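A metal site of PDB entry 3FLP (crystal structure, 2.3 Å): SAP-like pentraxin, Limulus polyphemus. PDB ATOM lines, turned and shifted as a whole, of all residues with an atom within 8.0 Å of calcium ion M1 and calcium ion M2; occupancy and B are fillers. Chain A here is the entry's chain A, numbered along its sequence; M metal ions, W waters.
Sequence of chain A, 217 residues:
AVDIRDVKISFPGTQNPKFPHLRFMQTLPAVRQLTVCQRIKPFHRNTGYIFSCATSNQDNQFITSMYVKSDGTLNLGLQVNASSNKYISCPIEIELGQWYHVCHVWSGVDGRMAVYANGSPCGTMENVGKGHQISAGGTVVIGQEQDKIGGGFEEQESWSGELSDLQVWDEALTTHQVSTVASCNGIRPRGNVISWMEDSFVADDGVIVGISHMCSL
OD1 of Asn 60 is bound to calcium ion M1 (2.3 Å).
Water W2 is bound to calcium ion M1 (2.3 Å).
Calcium ion M1 is bound by O of Gln 146, 2.4 Å away.
OD2 of Asp 59 is bound to calcium ion M1, 2.4 Å away.
OD1 of Asp 147 is bound to calcium ion M1.
The side-chain carboxylate (OE1) of Glu 145 is bound to calcium ion M1 (2.5 Å).
Calcium ion M1 is bound by OE2 of Glu 145 (2.6 Å).
Four residues have an atom within 4 Å of calcium ion M2: Glu 145, Asp 147, Glu 154 and Glu 157.
The nearest printed residue that does not touch calcium ion M2 is Gly 152 (4.4 Å).
Water W3 lies within hydrogen-bond range of O of Glu 145 (2.6 Å), O of Gly 152 (2.7 Å) and N of Glu 154 (3.2 Å).
The side-chain amide oxygen of Gln 79 sits at hydrogen-bond distance from the side-chain amide nitrogen of Asn 60, at 2.8 Å.
N of Asn 60 sits at hydrogen-bond distance from OE1 of Gln 58 (2.8 Å).
The backbone NH (N) of Tyr 49 sits at hydrogen-bond distance from the backbone carbonyl oxygen (O) of Glu 157 (3.0 Å).
The side-chain amide nitrogen of Gln 146 sits at hydrogen-bond distance from the backbone carbonyl oxygen of Ser 52 (2.8 Å).
Calcium ion M2 is bound by the side-chain carboxylate (OE1) of Glu 154, water W1, water W3, the side-chain carboxylate (OE1) of Glu 157, the side-chain carboxylate (OD2) of Asp 147, the side-chain carboxylate (OE1) of Glu 145 and the side-chain carboxylate (OD1) of Asp 147.
Calcium ion M2 has seven donor atoms within binding distance.
Within 4 Å of calcium ion M1: Asp 59, Asn 60, Glu 145, Gln 146 and Asp 147.
Along chain A the residues within 4 Å of calcium ion M1 span positions 59 to 147.
The nearest printed residue that does not touch calcium ion M1 is Ile 63 (5.1 Å).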
ATOM      1  N   TYR A  49      30.252 -32.407   2.169  1.00  0.00           N
ATOM      2  CA  TYR A  49      31.134 -31.390   1.586  1.00  0.00           C
ATOM      3  C   TYR A  49      31.319 -30.252   2.567  1.00  0.00           C
ATOM      4  O   TYR A  49      30.351 -29.679   3.075  1.00  0.00           O
ATOM      5  CB  TYR A  49      30.543 -30.881   0.268  1.00  0.00           C
ATOM      6  CG  TYR A  49      30.557 -31.952  -0.791  1.00  0.00           C
ATOM      7  CD1 TYR A  49      29.610 -32.976  -0.783  1.00  0.00           C
ATOM      8  CD2 TYR A  49      31.575 -32.006  -1.744  1.00  0.00           C
ATOM      9  CE1 TYR A  49      29.679 -34.029  -1.678  1.00  0.00           C
ATOM     10  CE2 TYR A  49      31.667 -33.060  -2.645  1.00  0.00           C
ATOM     11  CZ  TYR A  49      30.717 -34.067  -2.611  1.00  0.00           C
ATOM     12  OH  TYR A  49      30.811 -35.112  -3.489  1.00  0.00           O
ATOM     13  N   SER A  52      32.962 -25.332  -0.207  1.00  0.00           N
ATOM     14  CA  SER A  52      32.399 -25.280  -1.555  1.00  0.00           C
ATOM     15  C   SER A  52      32.583 -23.907  -2.199  1.00  0.00           C
ATOM     16  O   SER A  52      32.148 -22.900  -1.646  1.00  0.00           O
ATOM     17  CB  SER A  52      30.903 -25.634  -1.505  1.00  0.00           C
ATOM     18  OG  SER A  52      30.231 -25.323  -2.713  1.00  0.00           O
ATOM     19  N   CYS A  53      33.241 -23.872  -3.361  1.00  0.00           N
ATOM     20  CA  CYS A  53      33.477 -22.629  -4.082  1.00  0.00           C
ATOM     21  C   CYS A  53      32.809 -22.684  -5.459  1.00  0.00           C
ATOM     22  O   CYS A  53      33.035 -23.614  -6.226  1.00  0.00           O
ATOM     23  CB  CYS A  53      34.970 -22.379  -4.244  1.00  0.00           C
ATOM     24  SG  CYS A  53      35.332 -20.843  -5.125  1.00  0.00           S
ATOM     25  N   ALA A  54      32.000 -21.671  -5.762  1.00  0.00           N
ATOM     26  CA  ALA A  54      31.289 -21.643  -7.031  1.00  0.00           C
ATOM     27  C   ALA A  54      31.308 -20.286  -7.736  1.00  0.00           C
ATOM     28  O   ALA A  54      31.255 -19.250  -7.084  1.00  0.00           O
ATOM     29  CB  ALA A  54      29.853 -22.087  -6.814  1.00  0.00           C
ATOM     30  N   GLN A  58      30.429 -22.062 -13.142  1.00  0.00           N
ATOM     31  CA  GLN A  58      30.885 -23.337 -12.602  1.00  0.00           C
ATOM     32  C   GLN A  58      30.615 -23.458 -11.108  1.00  0.00           C
ATOM     33  O   GLN A  58      31.364 -22.927 -10.296  1.00  0.00           O
ATOM     34  CB  GLN A  58      32.394 -23.483 -12.864  1.00  0.00           C
ATOM     35  CG  GLN A  58      33.045 -24.751 -12.313  1.00  0.00           C
ATOM     36  CD  GLN A  58      32.327 -26.019 -12.743  1.00  0.00           C
ATOM     37  OE1 GLN A  58      31.390 -26.452 -12.092  1.00  0.00           O
ATOM     38  NE2 GLN A  58      32.759 -26.586 -13.868  1.00  0.00           N
ATOM     39  N   ASP A  59      29.541 -24.165 -10.758  1.00  0.00           N
ATOM     40  CA  ASP A  59      29.191 -24.327  -9.354  1.00  0.00           C
ATOM     41  C   ASP A  59      30.162 -25.226  -8.598  1.00  0.00           C
ATOM     42  O   ASP A  59      30.165 -25.237  -7.366  1.00  0.00           O
ATOM     43  CB  ASP A  59      27.754 -24.867  -9.226  1.00  0.00           C
ATOM     44  CG  ASP A  59      27.563 -26.247  -9.850  1.00  0.00           C
ATOM     45  OD1 ASP A  59      27.923 -26.439 -11.028  1.00  0.00           O
ATOM     46  OD2 ASP A  59      27.023 -27.144  -9.154  1.00  0.00           O
ATOM     47  N   ASN A  60      30.986 -25.964  -9.337  1.00  0.00           N
ATOM     48  CA  ASN A  60      31.940 -26.878  -8.725  1.00  0.00           C
ATOM     49  C   ASN A  60      33.410 -26.509  -8.998  1.00  0.00           C
ATOM     50  O   ASN A  60      34.194 -27.335  -9.463  1.00  0.00           O
ATOM     51  CB  ASN A  60      31.662 -28.307  -9.222  1.00  0.00           C
ATOM     52  CG  ASN A  60      30.318 -28.851  -8.706  1.00  0.00           C
ATOM     53  OD1 ASN A  60      29.446 -28.091  -8.276  1.00  0.00           O
ATOM     54  ND2 ASN A  60      30.152 -30.174  -8.761  1.00  0.00           N
ATOM     55  N   GLN A  61      33.768 -25.263  -8.712  1.00  0.00           N
ATOM     56  CA  GLN A  61      35.143 -24.800  -8.937  1.00  0.00           C
ATOM     57  C   GLN A  61      36.144 -25.504  -8.017  1.00  0.00           C
ATOM     58  O   GLN A  61      37.199 -25.949  -8.463  1.00  0.00           O
ATOM     59  CB  GLN A  61      35.221 -23.289  -8.724  1.00  0.00           C
ATOM     60  CG  GLN A  61      34.736 -22.469  -9.906  1.00  0.00           C
ATOM     61  CD  GLN A  61      35.761 -22.401 -11.036  1.00  0.00           C
ATOM     62  OE1 GLN A  61      36.750 -23.138 -11.045  1.00  0.00           O
ATOM     63  NE2 GLN A  61      35.534 -21.508 -11.987  1.00  0.00           N
ATOM     64  N   ILE A  63      35.866 -28.045  -4.355  1.00  0.00           N
ATOM     65  CA  ILE A  63      35.056 -28.587  -3.263  1.00  0.00           C
ATOM     66  C   ILE A  63      35.796 -29.657  -2.484  1.00  0.00           C
ATOM     67  O   ILE A  63      36.320 -30.623  -3.051  1.00  0.00           O
ATOM     68  CB  ILE A  63      33.741 -29.218  -3.777  1.00  0.00           C
ATOM     69  CG1 ILE A  63      33.457 -28.774  -5.217  1.00  0.00           C
ATOM     70  CG2 ILE A  63      32.592 -28.781  -2.878  1.00  0.00           C
ATOM     71  CD1 ILE A  63      32.238 -29.435  -5.823  1.00  0.00           C
ATOM     72  N   GLN A  79      37.572 -31.930  -5.370  1.00  0.00           N
ATOM     73  CA  GLN A  79      37.025 -31.841  -6.705  1.00  0.00           C
ATOM     74  C   GLN A  79      37.368 -30.445  -7.205  1.00  0.00           C
ATOM     75  O   GLN A  79      37.164 -29.461  -6.504  1.00  0.00           O
ATOM     76  CB  GLN A  79      35.502 -32.068  -6.691  1.00  0.00           C
ATOM     77  CG  GLN A  79      34.823 -31.687  -7.998  1.00  0.00           C
ATOM     78  CD  GLN A  79      33.356 -32.093  -8.083  1.00  0.00           C
ATOM     79  OE1 GLN A  79      32.608 -31.570  -8.913  1.00  0.00           O
ATOM     80  NE2 GLN A  79      32.950 -33.044  -7.247  1.00  0.00           N
ATOM     81  N   GLN A 144      27.650 -26.937   3.065  1.00  0.00           N
ATOM     82  CA  GLN A 144      26.718 -27.366   2.031  1.00  0.00           C
ATOM     83  C   GLN A 144      27.433 -27.329   0.681  1.00  0.00           C
ATOM     84  O   GLN A 144      28.445 -26.651   0.532  1.00  0.00           O
ATOM     85  CB  GLN A 144      25.481 -26.449   1.972  1.00  0.00           C
ATOM     86  CG  GLN A 144      24.638 -26.331   3.252  1.00  0.00           C
ATOM     87  CD  GLN A 144      23.948 -27.640   3.650  1.00  0.00           C
ATOM     88  OE1 GLN A 144      23.690 -28.506   2.821  1.00  0.00           O
ATOM     89  NE2 GLN A 144      23.636 -27.764   4.924  1.00  0.00           N
ATOM     90  N   GLU A 145      26.904 -28.066  -0.298  1.00  0.00           N
ATOM     91  CA  GLU A 145      27.467 -28.130  -1.642  1.00  0.00           C
ATOM     92  C   GLU A 145      26.599 -27.240  -2.538  1.00  0.00           C
ATOM     93  O   GLU A 145      25.389 -27.465  -2.638  1.00  0.00           O
ATOM     94  CB  GLU A 145      27.428 -29.590  -2.119  1.00  0.00           C
ATOM     95  CG  GLU A 145      28.473 -29.979  -3.174  1.00  0.00           C
ATOM     96  CD  GLU A 145      28.150 -29.473  -4.564  1.00  0.00           C
ATOM     97  OE1 GLU A 145      27.022 -29.738  -5.058  1.00  0.00           O
ATOM     98  OE2 GLU A 145      29.016 -28.803  -5.167  1.00  0.00           O
ATOM     99  N   GLN A 146      27.188 -26.232  -3.174  1.00  0.00           N
ATOM    100  CA  GLN A 146      26.442 -25.325  -4.050  1.00  0.00           C
ATOM    101  C   GLN A 146      26.193 -25.866  -5.457  1.00  0.00           C
ATOM    102  O   GLN A 146      27.092 -26.426  -6.082  1.00  0.00           O
ATOM    103  CB  GLN A 146      27.173 -23.994  -4.213  1.00  0.00           C
ATOM    104  CG  GLN A 146      27.488 -23.223  -2.943  1.00  0.00           C
ATOM    105  CD  GLN A 146      28.437 -22.056  -3.208  1.00  0.00           C
ATOM    106  OE1 GLN A 146      28.024 -20.979  -3.644  1.00  0.00           O
ATOM    107  NE2 GLN A 146      29.724 -22.278  -2.946  1.00  0.00           N
ATOM    108  N   ASP A 147      24.955 -25.705  -5.947  1.00  0.00           N
ATOM    109  CA  ASP A 147      24.602 -26.101  -7.305  1.00  0.00           C
ATOM    110  C   ASP A 147      24.262 -24.810  -8.028  1.00  0.00           C
ATOM    111  O   ASP A 147      23.975 -24.786  -9.221  1.00  0.00           O
ATOM    112  CB  ASP A 147      23.418 -27.069  -7.321  1.00  0.00           C
ATOM    113  CG  ASP A 147      23.818 -28.473  -6.942  1.00  0.00           C
ATOM    114  OD1 ASP A 147      25.001 -28.825  -7.158  1.00  0.00           O
ATOM    115  OD2 ASP A 147      22.960 -29.241  -6.458  1.00  0.00           O
ATOM    116  N   LYS A 148      24.309 -23.730  -7.249  1.00  0.00           N
ATOM    117  CA  LYS A 148      24.070 -22.371  -7.733  1.00  0.00           C
ATOM    118  C   LYS A 148      24.761 -21.481  -6.712  1.00  0.00           C
ATOM    119  O   LYS A 148      25.007 -21.900  -5.579  1.00  0.00           O
ATOM    120  CB  LYS A 148      22.577 -22.042  -7.788  1.00  0.00           C
ATOM    121  CG  LYS A 148      21.879 -22.148  -6.442  1.00  0.00           C
ATOM    122  CD  LYS A 148      20.620 -21.287  -6.362  1.00  0.00           C
ATOM    123  CE  LYS A 148      19.576 -21.688  -7.391  1.00  0.00           C
ATOM    124  NZ  LYS A 148      18.315 -20.942  -7.162  1.00  0.00           N
ATOM    125  N   GLY A 151      23.473 -21.331  -3.090  1.00  0.00           N
ATOM    126  CA  GLY A 151      22.275 -22.127  -2.916  1.00  0.00           C
ATOM    127  C   GLY A 151      22.244 -23.449  -3.660  1.00  0.00           C
ATOM    128  O   GLY A 151      23.290 -23.989  -4.028  1.00  0.00           O
ATOM    129  N   GLY A 152      21.039 -23.960  -3.887  1.00  0.00           N
ATOM    130  CA  GLY A 152      20.861 -25.234  -4.576  1.00  0.00           C
ATOM    131  C   GLY A 152      21.454 -26.364  -3.758  1.00  0.00           C
ATOM    132  O   GLY A 152      22.008 -27.310  -4.302  1.00  0.00           O
ATOM    133  N   PHE A 153      21.320 -26.262  -2.440  1.00  0.00           N
ATOM    134  CA  PHE A 153      21.853 -27.260  -1.516  1.00  0.00           C
ATOM    135  C   PHE A 153      21.076 -28.577  -1.549  1.00  0.00           C
ATOM    136  O   PHE A 153      19.889 -28.614  -1.848  1.00  0.00           O
ATOM    137  CB  PHE A 153      21.841 -26.727  -0.081  1.00  0.00           C
ATOM    138  CG  PHE A 153      22.552 -25.406   0.087  1.00  0.00           C
ATOM    139  CD1 PHE A 153      23.753 -25.168  -0.560  1.00  0.00           C
ATOM    140  CD2 PHE A 153      22.012 -24.423   0.898  1.00  0.00           C
ATOM    141  CE1 PHE A 153      24.416 -23.943  -0.406  1.00  0.00           C
ATOM    142  CE2 PHE A 153      22.668 -23.194   1.072  1.00  0.00           C
ATOM    143  CZ  PHE A 153      23.875 -22.961   0.414  1.00  0.00           C
ATOM    144  N   GLU A 154      21.771 -29.667  -1.217  1.00  0.00           N
ATOM    145  CA  GLU A 154      21.182 -31.003  -1.184  1.00  0.00           C
ATOM    146  C   GLU A 154      21.557 -31.672   0.131  1.00  0.00           C
ATOM    147  O   GLU A 154      22.743 -31.754   0.472  1.00  0.00           O
ATOM    148  CB  GLU A 154      21.693 -31.847  -2.365  1.00  0.00           C
ATOM    149  CG  GLU A 154      21.180 -31.376  -3.709  1.00  0.00           C
ATOM    150  CD  GLU A 154      21.710 -32.206  -4.861  1.00  0.00           C
ATOM    151  OE1 GLU A 154      22.913 -32.075  -5.198  1.00  0.00           O
ATOM    152  OE2 GLU A 154      20.928 -32.991  -5.430  1.00  0.00           O
ATOM    153  N   GLU A 155      20.561 -32.155   0.852  1.00  0.00           N
ATOM    154  CA  GLU A 155      20.810 -32.778   2.153  1.00  0.00           C
ATOM    155  C   GLU A 155      21.811 -33.931   2.153  1.00  0.00           C
ATOM    156  O   GLU A 155      22.568 -34.083   3.104  1.00  0.00           O
ATOM    157  CB  GLU A 155      19.489 -33.203   2.810  1.00  0.00           C
ATOM    158  CG  GLU A 155      18.568 -34.068   1.959  1.00  0.00           C
ATOM    159  CD  GLU A 155      17.226 -34.353   2.649  1.00  0.00           C
ATOM    160  OE1 GLU A 155      16.499 -33.385   3.006  1.00  0.00           O
ATOM    161  OE2 GLU A 155      16.885 -35.549   2.823  1.00  0.00           O
ATOM    162  N   GLN A 156      21.825 -34.736   1.090  1.00  0.00           N
ATOM    163  CA  GLN A 156      22.760 -35.855   1.043  1.00  0.00           C
ATOM    164  C   GLN A 156      24.220 -35.444   0.822  1.00  0.00           C
ATOM    165  O   GLN A 156      25.114 -36.272   0.906  1.00  0.00           O
ATOM    166  CB  GLN A 156      22.329 -36.867  -0.019  1.00  0.00           C
ATOM    167  CG  GLN A 156      21.095 -37.677   0.397  1.00  0.00           C
ATOM    168  CD  GLN A 156      20.782 -38.807  -0.577  1.00  0.00           C
ATOM    169  OE1 GLN A 156      20.474 -38.562  -1.758  1.00  0.00           O
ATOM    170  NE2 GLN A 156      20.841 -40.047  -0.089  1.00  0.00           N
ATOM    171  N   GLU A 157      24.461 -34.164   0.544  1.00  0.00           N
ATOM    172  CA  GLU A 157      25.823 -33.687   0.341  1.00  0.00           C
ATOM    173  C   GLU A 157      26.259 -32.713   1.437  1.00  0.00           C
ATOM    174  O   GLU A 157      27.365 -32.153   1.382  1.00  0.00           O
ATOM    175  CB  GLU A 157      25.942 -33.035  -1.034  1.00  0.00           C
ATOM    176  CG  GLU A 157      25.641 -33.996  -2.183  1.00  0.00           C
ATOM    177  CD  GLU A 157      25.668 -33.318  -3.549  1.00  0.00           C
ATOM    178  OE1 GLU A 157      25.055 -32.248  -3.691  1.00  0.00           O
ATOM    179  OE2 GLU A 157      26.282 -33.873  -4.485  1.00  0.00           O
HETATM  180 CA    CA M   1      27.402 -28.506  -7.207  1.00  0.00          CA
HETATM  181 CA    CA M   2      24.666 -30.596  -5.352  1.00  0.00          CA
HETATM  182  O   HOH W   1      25.725 -32.352  -6.521  1.00  0.00           O
HETATM  183  O   HOH W   2      27.287 -30.753  -7.864  1.00  0.00           O
HETATM  184  O   HOH W   3      23.795 -29.218  -3.631  1.00  0.00           O
